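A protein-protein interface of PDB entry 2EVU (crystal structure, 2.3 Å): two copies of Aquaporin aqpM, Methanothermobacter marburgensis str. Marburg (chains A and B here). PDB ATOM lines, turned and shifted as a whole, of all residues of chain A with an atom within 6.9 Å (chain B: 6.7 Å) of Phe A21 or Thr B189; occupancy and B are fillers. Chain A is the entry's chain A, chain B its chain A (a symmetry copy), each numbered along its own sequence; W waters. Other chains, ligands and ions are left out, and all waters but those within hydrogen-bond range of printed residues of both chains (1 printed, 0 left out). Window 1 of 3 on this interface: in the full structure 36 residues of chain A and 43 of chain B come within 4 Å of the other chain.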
ATOM      1  N   THR A  15      33.767  17.705 -14.046  1.00  0.00           N
ATOM      2  CA  THR A  15      32.386  17.913 -13.635  1.00  0.00           C
ATOM      3  C   THR A  15      31.515  16.804 -14.242  1.00  0.00           C
ATOM      4  O   THR A  15      30.510  16.400 -13.651  1.00  0.00           O
ATOM      5  CB  THR A  15      31.874  19.288 -14.079  1.00  0.00           C
ATOM      6  OG1 THR A  15      32.922  20.254 -13.913  1.00  0.00           O
ATOM      7  CG2 THR A  15      30.685  19.712 -13.217  1.00  0.00           C
ATOM      8  N   PHE A  16      31.916  16.305 -15.411  1.00  0.00           N
ATOM      9  CA  PHE A  16      31.184  15.221 -16.068  1.00  0.00           C
ATOM     10  C   PHE A  16      31.224  14.001 -15.150  1.00  0.00           C
ATOM     11  O   PHE A  16      30.194  13.390 -14.844  1.00  0.00           O
ATOM     12  CB  PHE A  16      31.833  14.889 -17.426  1.00  0.00           C
ATOM     13  CG  PHE A  16      31.301  13.628 -18.084  1.00  0.00           C
ATOM     14  CD1 PHE A  16      31.679  12.365 -17.626  1.00  0.00           C
ATOM     15  CD2 PHE A  16      30.428  13.707 -19.165  1.00  0.00           C
ATOM     16  CE1 PHE A  16      31.191  11.198 -18.235  1.00  0.00           C
ATOM     17  CE2 PHE A  16      29.939  12.554 -19.779  1.00  0.00           C
ATOM     18  CZ  PHE A  16      30.320  11.295 -19.311  1.00  0.00           C
ATOM     19  N   ILE A  17      32.432  13.662 -14.711  1.00  0.00           N
ATOM     20  CA  ILE A  17      32.655  12.529 -13.826  1.00  0.00           C
ATOM     21  C   ILE A  17      31.864  12.690 -12.540  1.00  0.00           C
ATOM     22  O   ILE A  17      31.206  11.755 -12.068  1.00  0.00           O
ATOM     23  CB  ILE A  17      34.154  12.406 -13.492  1.00  0.00           C
ATOM     24  CG1 ILE A  17      34.919  12.012 -14.756  1.00  0.00           C
ATOM     25  CG2 ILE A  17      34.371  11.394 -12.367  1.00  0.00           C
ATOM     26  CD1 ILE A  17      36.422  12.119 -14.622  1.00  0.00           C
ATOM     27  N   LEU A  18      31.931  13.891 -11.980  1.00  0.00           N
ATOM     28  CA  LEU A  18      31.236  14.209 -10.741  1.00  0.00           C
ATOM     29  C   LEU A  18      29.736  13.930 -10.808  1.00  0.00           C
ATOM     30  O   LEU A  18      29.172  13.258  -9.938  1.00  0.00           O
ATOM     31  CB  LEU A  18      31.484  15.675 -10.402  1.00  0.00           C
ATOM     32  CG  LEU A  18      30.932  16.277  -9.114  1.00  0.00           C
ATOM     33  CD1 LEU A  18      31.763  17.487  -8.780  1.00  0.00           C
ATOM     34  CD2 LEU A  18      29.476  16.661  -9.269  1.00  0.00           C
ATOM     35  N   VAL A  19      29.090  14.451 -11.842  1.00  0.00           N
ATOM     36  CA  VAL A  19      27.657  14.270 -11.997  1.00  0.00           C
ATOM     37  C   VAL A  19      27.320  12.850 -12.440  1.00  0.00           C
ATOM     38  O   VAL A  19      26.370  12.250 -11.944  1.00  0.00           O
ATOM     39  CB  VAL A  19      27.082  15.304 -13.007  1.00  0.00           C
ATOM     40  CG1 VAL A  19      25.584  15.068 -13.224  1.00  0.00           C
ATOM     41  CG2 VAL A  19      27.319  16.717 -12.479  1.00  0.00           C
ATOM     42  N   PHE A  20      28.103  12.305 -13.358  1.00  0.00           N
ATOM     43  CA  PHE A  20      27.844  10.955 -13.831  1.00  0.00           C
ATOM     44  C   PHE A  20      27.843   9.952 -12.680  1.00  0.00           C
ATOM     45  O   PHE A  20      26.874   9.211 -12.485  1.00  0.00           O
ATOM     46  CB  PHE A  20      28.890  10.544 -14.875  1.00  0.00           C
ATOM     47  CG  PHE A  20      28.659   9.178 -15.454  1.00  0.00           C
ATOM     48  CD1 PHE A  20      29.046   8.033 -14.756  1.00  0.00           C
ATOM     49  CD2 PHE A  20      28.021   9.030 -16.683  1.00  0.00           C
ATOM     50  CE1 PHE A  20      28.798   6.762 -15.271  1.00  0.00           C
ATOM     51  CE2 PHE A  20      27.766   7.760 -17.208  1.00  0.00           C
ATOM     52  CZ  PHE A  20      28.154   6.625 -16.501  1.00  0.00           C
ATOM     53  N   PHE A  21      28.927   9.943 -11.912  1.00  0.00           N
ATOM     54  CA  PHE A  21      29.071   9.016 -10.800  1.00  0.00           C
ATOM     55  C   PHE A  21      28.312   9.366  -9.524  1.00  0.00           C
ATOM     56  O   PHE A  21      27.642   8.506  -8.947  1.00  0.00           O
ATOM     57  CB  PHE A  21      30.560   8.814 -10.517  1.00  0.00           C
ATOM     58  CG  PHE A  21      31.266   8.051 -11.603  1.00  0.00           C
ATOM     59  CD1 PHE A  21      31.080   6.673 -11.735  1.00  0.00           C
ATOM     60  CD2 PHE A  21      32.048   8.716 -12.546  1.00  0.00           C
ATOM     61  CE1 PHE A  21      31.657   5.962 -12.795  1.00  0.00           C
ATOM     62  CE2 PHE A  21      32.629   8.019 -13.609  1.00  0.00           C
ATOM     63  CZ  PHE A  21      32.434   6.638 -13.736  1.00  0.00           C
ATOM     64  N   GLY A  22      28.395  10.618  -9.089  1.00  0.00           N
ATOM     65  CA  GLY A  22      27.699  11.015  -7.882  1.00  0.00           C
ATOM     66  C   GLY A  22      26.187  10.977  -8.034  1.00  0.00           C
ATOM     67  O   GLY A  22      25.504  10.173  -7.392  1.00  0.00           O
ATOM     68  N   ALA A  23      25.657  11.850  -8.887  1.00  0.00           N
ATOM     69  CA  ALA A  23      24.221  11.914  -9.111  1.00  0.00           C
ATOM     70  C   ALA A  23      23.705  10.570  -9.593  1.00  0.00           C
ATOM     71  O   ALA A  23      22.560  10.203  -9.323  1.00  0.00           O
ATOM     72  CB  ALA A  23      23.897  12.994 -10.128  1.00  0.00           C
ATOM     73  N   GLY A  24      24.558   9.835 -10.305  1.00  0.00           N
ATOM     74  CA  GLY A  24      24.162   8.537 -10.810  1.00  0.00           C
ATOM     75  C   GLY A  24      23.818   7.554  -9.704  1.00  0.00           C
ATOM     76  O   GLY A  24      22.843   6.806  -9.815  1.00  0.00           O
ATOM     77  N   SER A  25      24.607   7.553  -8.632  1.00  0.00           N
ATOM     78  CA  SER A  25      24.372   6.632  -7.521  1.00  0.00           C
ATOM     79  C   SER A  25      23.053   6.933  -6.834  1.00  0.00           C
ATOM     80  O   SER A  25      22.364   6.025  -6.377  1.00  0.00           O
ATOM     81  CB  SER A  25      25.512   6.706  -6.496  1.00  0.00           C
ATOM     82  OG  SER A  25      25.564   7.979  -5.863  1.00  0.00           O
ATOM     83  N   ALA A  26      22.705   8.212  -6.762  1.00  0.00           N
ATOM     84  CA  ALA A  26      21.450   8.618  -6.135  1.00  0.00           C
ATOM     85  C   ALA A  26      20.288   8.068  -6.962  1.00  0.00           C
ATOM     86  O   ALA A  26      19.358   7.470  -6.421  1.00  0.00           O
ATOM     87  CB  ALA A  26      21.370  10.152  -6.049  1.00  0.00           C
ATOM     88  N   VAL A  28      20.279   5.573  -9.138  1.00  0.00           N
ATOM     89  CA  VAL A  28      20.289   4.119  -9.044  1.00  0.00           C
ATOM     90  C   VAL A  28      19.664   3.632  -7.739  1.00  0.00           C
ATOM     91  O   VAL A  28      18.962   2.630  -7.723  1.00  0.00           O
ATOM     92  CB  VAL A  28      21.739   3.577  -9.159  1.00  0.00           C
ATOM     93  CG1 VAL A  28      21.804   2.111  -8.723  1.00  0.00           C
ATOM     94  CG2 VAL A  28      22.222   3.717 -10.592  1.00  0.00           C
ATOM     95  N   ILE A  58      25.963   7.073  -1.256  1.00  0.00           N
ATOM     96  CA  ILE A  58      25.841   8.110  -2.271  1.00  0.00           C
ATOM     97  C   ILE A  58      26.943   9.157  -2.049  1.00  0.00           C
ATOM     98  O   ILE A  58      27.585   9.618  -2.997  1.00  0.00           O
ATOM     99  CB  ILE A  58      24.443   8.789  -2.198  1.00  0.00           C
ATOM    100  CG1 ILE A  58      23.366   7.795  -2.653  1.00  0.00           C
ATOM    101  CG2 ILE A  58      24.425  10.067  -3.057  1.00  0.00           C
ATOM    102  CD1 ILE A  58      21.944   8.267  -2.403  1.00  0.00           C
ATOM    103  N   ALA A  61      30.162   7.804  -3.326  1.00  0.00           N
ATOM    104  CA  ALA A  61      30.220   7.723  -4.779  1.00  0.00           C
ATOM    105  C   ALA A  61      30.658   9.097  -5.284  1.00  0.00           C
ATOM    106  O   ALA A  61      31.406   9.215  -6.256  1.00  0.00           O
ATOM    107  CB  ALA A  61      28.862   7.346  -5.344  1.00  0.00           C
ATOM    108  N   PHE A  62      30.188  10.139  -4.607  1.00  0.00           N
ATOM    109  CA  PHE A  62      30.558  11.507  -4.947  1.00  0.00           C
ATOM    110  C   PHE A  62      32.009  11.733  -4.551  1.00  0.00           C
ATOM    111  O   PHE A  62      32.829  12.174  -5.357  1.00  0.00           O
ATOM    112  CB  PHE A  62      29.683  12.503  -4.178  1.00  0.00           C
ATOM    113  CG  PHE A  62      28.465  12.945  -4.927  1.00  0.00           C
ATOM    114  CD1 PHE A  62      28.570  13.887  -5.942  1.00  0.00           C
ATOM    115  CD2 PHE A  62      27.210  12.399  -4.635  1.00  0.00           C
ATOM    116  CE1 PHE A  62      27.439  14.288  -6.664  1.00  0.00           C
ATOM    117  CE2 PHE A  62      26.075  12.790  -5.348  1.00  0.00           C
ATOM    118  CZ  PHE A  62      26.192  13.740  -6.369  1.00  0.00           C
ATOM    119  N   ALA A  65      34.763   9.796  -6.485  1.00  0.00           N
ATOM    120  CA  ALA A  65      34.824  10.295  -7.853  1.00  0.00           C
ATOM    121  C   ALA A  65      35.531  11.643  -7.847  1.00  0.00           C
ATOM    122  O   ALA A  65      36.323  11.953  -8.742  1.00  0.00           O
ATOM    123  CB  ALA A  65      33.413  10.437  -8.427  1.00  0.00           C
ATOM    124  N   GLY A 114      27.424  15.033 -18.522  1.00  0.00           N
ATOM    125  CA  GLY A 114      27.617  13.888 -17.649  1.00  0.00           C
ATOM    126  C   GLY A 114      26.296  13.247 -17.267  1.00  0.00           C
ATOM    127  O   GLY A 114      26.170  12.022 -17.229  1.00  0.00           O
ATOM    128  N   PHE A 118      24.813   9.403 -18.498  1.00  0.00           N
ATOM    129  CA  PHE A 118      24.403   8.440 -17.487  1.00  0.00           C
ATOM    130  C   PHE A 118      22.985   7.990 -17.802  1.00  0.00           C
ATOM    131  O   PHE A 118      22.651   6.813 -17.672  1.00  0.00           O
ATOM    132  CB  PHE A 118      24.441   9.042 -16.082  1.00  0.00           C
ATOM    133  CG  PHE A 118      24.011   8.080 -15.019  1.00  0.00           C
ATOM    134  CD1 PHE A 118      24.863   7.063 -14.601  1.00  0.00           C
ATOM    135  CD2 PHE A 118      22.728   8.140 -14.485  1.00  0.00           C
ATOM    136  CE1 PHE A 118      24.442   6.112 -13.663  1.00  0.00           C
ATOM    137  CE2 PHE A 118      22.296   7.200 -13.553  1.00  0.00           C
ATOM    138  CZ  PHE A 118      23.160   6.179 -13.141  1.00  0.00           C
ATOM    139  N   LEU B  52      21.834   0.797  -1.443  1.00  0.00           N
ATOM    140  CA  LEU B  52      23.091   1.138  -2.100  1.00  0.00           C
ATOM    141  C   LEU B  52      24.235   0.767  -1.155  1.00  0.00           C
ATOM    142  O   LEU B  52      25.375   0.588  -1.586  1.00  0.00           O
ATOM    143  CB  LEU B  52      23.158   2.630  -2.433  1.00  0.00           C
ATOM    144  CG  LEU B  52      24.211   2.956  -3.497  1.00  0.00           C
ATOM    145  CD1 LEU B  52      23.821   2.259  -4.805  1.00  0.00           C
ATOM    146  CD2 LEU B  52      24.327   4.466  -3.704  1.00  0.00           C
ATOM    147  N   TRP B  55      26.044  -2.070  -2.326  1.00  0.00           N
ATOM    148  CA  TRP B  55      26.920  -1.806  -3.458  1.00  0.00           C
ATOM    149  C   TRP B  55      28.229  -1.138  -3.030  1.00  0.00           C
ATOM    150  O   TRP B  55      29.285  -1.421  -3.593  1.00  0.00           O
ATOM    151  CB  TRP B  55      26.200  -0.948  -4.503  1.00  0.00           C
ATOM    152  CG  TRP B  55      25.350  -1.766  -5.448  1.00  0.00           C
ATOM    153  CD1 TRP B  55      23.987  -1.708  -5.601  1.00  0.00           C
ATOM    154  CD2 TRP B  55      25.814  -2.774  -6.356  1.00  0.00           C
ATOM    155  NE1 TRP B  55      23.580  -2.620  -6.548  1.00  0.00           N
ATOM    156  CE2 TRP B  55      24.677  -3.286  -7.027  1.00  0.00           C
ATOM    157  CE3 TRP B  55      27.078  -3.294  -6.666  1.00  0.00           C
ATOM    158  CZ2 TRP B  55      24.770  -4.295  -7.993  1.00  0.00           C
ATOM    159  CZ3 TRP B  55      27.168  -4.300  -7.631  1.00  0.00           C
ATOM    160  CH2 TRP B  55      26.019  -4.788  -8.281  1.00  0.00           C
ATOM    161  N   ALA B 149      28.626   1.960 -20.032  1.00  0.00           N
ATOM    162  CA  ALA B 149      28.927   2.046 -18.610  1.00  0.00           C
ATOM    163  C   ALA B 149      30.362   1.591 -18.358  1.00  0.00           C
ATOM    164  O   ALA B 149      31.101   2.209 -17.596  1.00  0.00           O
ATOM    165  CB  ALA B 149      27.952   1.174 -17.817  1.00  0.00           C
ATOM    166  N   VAL B 152      32.937   4.302 -19.721  1.00  0.00           N
ATOM    167  CA  VAL B 152      32.981   5.492 -18.880  1.00  0.00           C
ATOM    168  C   VAL B 152      33.641   5.134 -17.540  1.00  0.00           C
ATOM    169  O   VAL B 152      34.462   5.890 -17.012  1.00  0.00           O
ATOM    170  CB  VAL B 152      31.571   6.054 -18.622  1.00  0.00           C
ATOM    171  CG1 VAL B 152      31.642   7.179 -17.594  1.00  0.00           C
ATOM    172  CG2 VAL B 152      30.971   6.579 -19.931  1.00  0.00           C
ATOM    173  N   GLY B 153      33.289   3.966 -17.009  1.00  0.00           N
ATOM    174  CA  GLY B 153      33.863   3.518 -15.757  1.00  0.00           C
ATOM    175  C   GLY B 153      35.362   3.294 -15.860  1.00  0.00           C
ATOM    176  O   GLY B 153      36.134   3.813 -15.060  1.00  0.00           O
ATOM    177  N   THR B 154      35.789   2.525 -16.853  1.00  0.00           N
ATOM    178  CA  THR B 154      37.210   2.252 -17.012  1.00  0.00           C
ATOM    179  C   THR B 154      37.962   3.525 -17.391  1.00  0.00           C
ATOM    180  O   THR B 154      39.161   3.647 -17.151  1.00  0.00           O
ATOM    181  CB  THR B 154      37.446   1.170 -18.069  1.00  0.00           C
ATOM    182  OG1 THR B 154      36.544   0.082 -17.834  1.00  0.00           O
ATOM    183  CG2 THR B 154      38.875   0.644 -17.982  1.00  0.00           C
ATOM    184  N   LEU B 156      37.448   6.447 -16.068  1.00  0.00           N
ATOM    185  CA  LEU B 156      37.781   7.086 -14.804  1.00  0.00           C
ATOM    186  C   LEU B 156      38.942   6.359 -14.120  1.00  0.00           C
ATOM    187  O   LEU B 156      39.896   6.984 -13.660  1.00  0.00           O
ATOM    188  CB  LEU B 156      36.556   7.113 -13.875  1.00  0.00           C
ATOM    189  CG  LEU B 156      36.785   7.786 -12.515  1.00  0.00           C
ATOM    190  CD1 LEU B 156      37.320   9.204 -12.720  1.00  0.00           C
ATOM    191  CD2 LEU B 156      35.491   7.803 -11.716  1.00  0.00           C
ATOM    192  N   LEU B 157      38.856   5.035 -14.057  1.00  0.00           N
ATOM    193  CA  LEU B 157      39.902   4.240 -13.428  1.00  0.00           C
ATOM    194  C   LEU B 157      41.269   4.549 -14.021  1.00  0.00           C
ATOM    195  O   LEU B 157      42.230   4.829 -13.293  1.00  0.00           O
ATOM    196  CB  LEU B 157      39.603   2.753 -13.598  1.00  0.00           C
ATOM    197  CG  LEU B 157      40.713   1.744 -13.266  1.00  0.00           C
ATOM    198  CD1 LEU B 157      41.180   1.895 -11.811  1.00  0.00           C
ATOM    199  CD2 LEU B 157      40.182   0.341 -13.503  1.00  0.00           C
ATOM    200  N   ALA B 184      36.064   1.457  -5.991  1.00  0.00           N
ATOM    201  CA  ALA B 184      34.937   1.308  -5.068  1.00  0.00           C
ATOM    202  C   ALA B 184      33.822   2.266  -5.441  1.00  0.00           C
ATOM    203  O   ALA B 184      32.643   1.924  -5.344  1.00  0.00           O
ATOM    204  CB  ALA B 184      35.376   1.583  -3.647  1.00  0.00           C
ATOM    205  N   GLY B 185      34.200   3.469  -5.869  1.00  0.00           N
ATOM    206  CA  GLY B 185      33.205   4.459  -6.236  1.00  0.00           C
ATOM    207  C   GLY B 185      32.499   4.156  -7.543  1.00  0.00           C
ATOM    208  O   GLY B 185      31.294   4.366  -7.665  1.00  0.00           O
ATOM    209  N   ILE B 186      33.256   3.683  -8.526  1.00  0.00           N
ATOM    210  CA  ILE B 186      32.705   3.340  -9.832  1.00  0.00           C
ATOM    211  C   ILE B 186      31.711   2.188  -9.670  1.00  0.00           C
ATOM    212  O   ILE B 186      30.622   2.214 -10.239  1.00  0.00           O
ATOM    213  CB  ILE B 186      33.838   2.930 -10.810  1.00  0.00           C
ATOM    214  CG1 ILE B 186      34.729   4.147 -11.092  1.00  0.00           C
ATOM    215  CG2 ILE B 186      33.253   2.374 -12.111  1.00  0.00           C
ATOM    216  CD1 ILE B 186      36.083   3.790 -11.682  1.00  0.00           C
ATOM    217  N   ILE B 187      32.084   1.192  -8.871  1.00  0.00           N
ATOM    218  CA  ILE B 187      31.220   0.044  -8.623  1.00  0.00           C
ATOM    219  C   ILE B 187      29.947   0.444  -7.893  1.00  0.00           C
ATOM    220  O   ILE B 187      28.891  -0.152  -8.103  1.00  0.00           O
ATOM    221  CB  ILE B 187      31.935  -1.023  -7.773  1.00  0.00           C
ATOM    222  CG1 ILE B 187      33.068  -1.657  -8.584  1.00  0.00           C
ATOM    223  CG2 ILE B 187      30.931  -2.070  -7.295  1.00  0.00           C
ATOM    224  CD1 ILE B 187      33.868  -2.702  -7.811  1.00  0.00           C
ATOM    225  N   THR B 188      30.035   1.452  -7.035  1.00  0.00           N
ATOM    226  CA  THR B 188      28.858   1.872  -6.294  1.00  0.00           C
ATOM    227  C   THR B 188      27.760   2.375  -7.219  1.00  0.00           C
ATOM    228  O   THR B 188      26.589   2.073  -7.012  1.00  0.00           O
ATOM    229  CB  THR B 188      29.201   2.960  -5.260  1.00  0.00           C
ATOM    230  OG1 THR B 188      30.176   2.451  -4.345  1.00  0.00           O
ATOM    231  CG2 THR B 188      27.957   3.363  -4.469  1.00  0.00           C
ATOM    232  N   THR B 189      28.118   3.135  -8.246  1.00  0.00           N
ATOM    233  CA  THR B 189      27.088   3.630  -9.140  1.00  0.00           C
ATOM    234  C   THR B 189      26.829   2.752 -10.366  1.00  0.00           C
ATOM    235  O   THR B 189      25.686   2.544 -10.748  1.00  0.00           O
ATOM    236  CB  THR B 189      27.382   5.090  -9.590  1.00  0.00           C
ATOM    237  OG1 THR B 189      27.381   5.163 -11.020  1.00  0.00           O
ATOM    238  CG2 THR B 189      28.707   5.578  -9.041  1.00  0.00           C
ATOM    239  N   LEU B 190      27.880   2.207 -10.955  1.00  0.00           N
ATOM    240  CA  LEU B 190      27.733   1.386 -12.151  1.00  0.00           C
ATOM    241  C   LEU B 190      27.497  -0.104 -11.923  1.00  0.00           C
ATOM    242  O   LEU B 190      27.263  -0.845 -12.867  1.00  0.00           O
ATOM    243  CB  LEU B 190      28.956   1.584 -13.051  1.00  0.00           C
ATOM    244  CG  LEU B 190      28.788   2.462 -14.302  1.00  0.00           C
ATOM    245  CD1 LEU B 190      27.721   3.518 -14.107  1.00  0.00           C
ATOM    246  CD2 LEU B 190      30.125   3.080 -14.638  1.00  0.00           C
ATOM    247  N   GLY B 191      27.542  -0.541 -10.672  1.00  0.00           N
ATOM    248  CA  GLY B 191      27.344  -1.949 -10.383  1.00  0.00           C
ATOM    249  C   GLY B 191      25.993  -2.517 -10.793  1.00  0.00           C
ATOM    250  O   GLY B 191      25.920  -3.565 -11.435  1.00  0.00           O
ATOM    251  N   ASN B 192      24.919  -1.834 -10.420  1.00  0.00           N
ATOM    252  CA  ASN B 192      23.581  -2.308 -10.744  1.00  0.00           C
ATOM    253  C   ASN B 192      23.194  -2.001 -12.183  1.00  0.00           C
ATOM    254  O   ASN B 192      22.013  -1.974 -12.516  1.00  0.00           O
ATOM    255  CB  ASN B 192      22.545  -1.686  -9.802  1.00  0.00           C
ATOM    256  CG  ASN B 192      21.468  -2.673  -9.393  1.00  0.00           C
ATOM    257  OD1 ASN B 192      21.544  -3.287  -8.325  1.00  0.00           O
ATOM    258  ND2 ASN B 192      20.467  -2.849 -10.253  1.00  0.00           N
ATOM    259  N   ILE B 193      24.185  -1.748 -13.031  1.00  0.00           N
ATOM    260  CA  ILE B 193      23.915  -1.479 -14.436  1.00  0.00           C
ATOM    261  C   ILE B 193      24.608  -2.521 -15.299  1.00  0.00           C
ATOM    262  O   ILE B 193      23.969  -3.166 -16.132  1.00  0.00           O
ATOM    263  CB  ILE B 193      24.373  -0.058 -14.851  1.00  0.00           C
ATOM    264  CG1 ILE B 193      23.419   0.975 -14.241  1.00  0.00           C
ATOM    265  CG2 ILE B 193      24.396   0.072 -16.381  1.00  0.00           C
ATOM    266  CD1 ILE B 193      23.697   2.406 -14.653  1.00  0.00           C
ATOM    267  N   SER B 196      29.802  -3.443 -13.216  1.00  0.00           N
ATOM    268  CA  SER B 196      31.039  -2.667 -13.085  1.00  0.00           C
ATOM    269  C   SER B 196      32.319  -3.509 -13.041  1.00  0.00           C
ATOM    270  O   SER B 196      33.034  -3.533 -12.030  1.00  0.00           O
ATOM    271  CB  SER B 196      30.953  -1.782 -11.835  1.00  0.00           C
ATOM    272  OG  SER B 196      32.041  -0.880 -11.757  1.00  0.00           O
HETATM  273  O   HOH W   1      32.187   7.310  -7.735  1.00  0.00           O
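No position is printed for both chains. Of the 14 pairs that touch across the chains among the printed residues, none has its exchanged pair printed and touching as well.
Of the 19 printed residues of chain A, 7 touch a printed residue of chain B. Hydrophobic or aromatic side chains of chain A within 4 Å of the printed part of chain B: Ile A17, Phe A20, Phe A21, Val A28, Ile A58 and Phe A118. Of the 19 printed residues of chain B, 8 touch a printed residue of chain A. Along chain B the printed residues that touch a printed residue of chain A span positions 52 to 193. Among the printed residues, 14 pairs touch across the chains.
Thr B189 touches just these residues of chain A: Phe A21, Ser A25 and Val A28. Of the printed residues of chain B, Ile A58 touches Leu B52 (3.6 Å). Of the printed residues of chain A, Leu B52 touches Ser A25 (3.7 Å) and Ile A58 (3.6 Å). The nearest printed residue of chain B that does not touch Phe A21 is Gly B185 (4.7 Å).
Water W1 bridges the backbone carbonyl oxygen (O) of Ala A61 (2.5 Å) and the backbone carbonyl oxygen (O) of Gly B185 (3.1 Å).
Among the printed residues, pairs that only touch across the chains: Ile A17 with Leu B156 (3.6 Å), Phe A20 with Val B152 (3.7 Å), Phe A20 with Leu B190 (3.6 Å), Phe A21 with Val B152 (3.9 Å), Phe A21 with Gly B153 (3.98 Å), Phe A21 with Leu B156 (3.4 Å), Phe A21 with Ile B186 (3.95 Å), Phe A21 with Thr B189 (3.1 Å), Phe A21 with Leu B190 (3.7 Å), Ser A25 with Leu B52 (3.7 Å), Ser A25 with Thr B189 (3.8 Å), Val A28 with Thr B189 (3.7 Å), Ile A58 with Leu B52 (3.6 Å) and Phe A118 with Ile B193 (3.9 Å).
The side-chain hydroxyl (OG) of Ser A25 is in hydrogen-bond range of the backbone carbonyl oxygen (O) of Gly A22 (2.7 Å).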
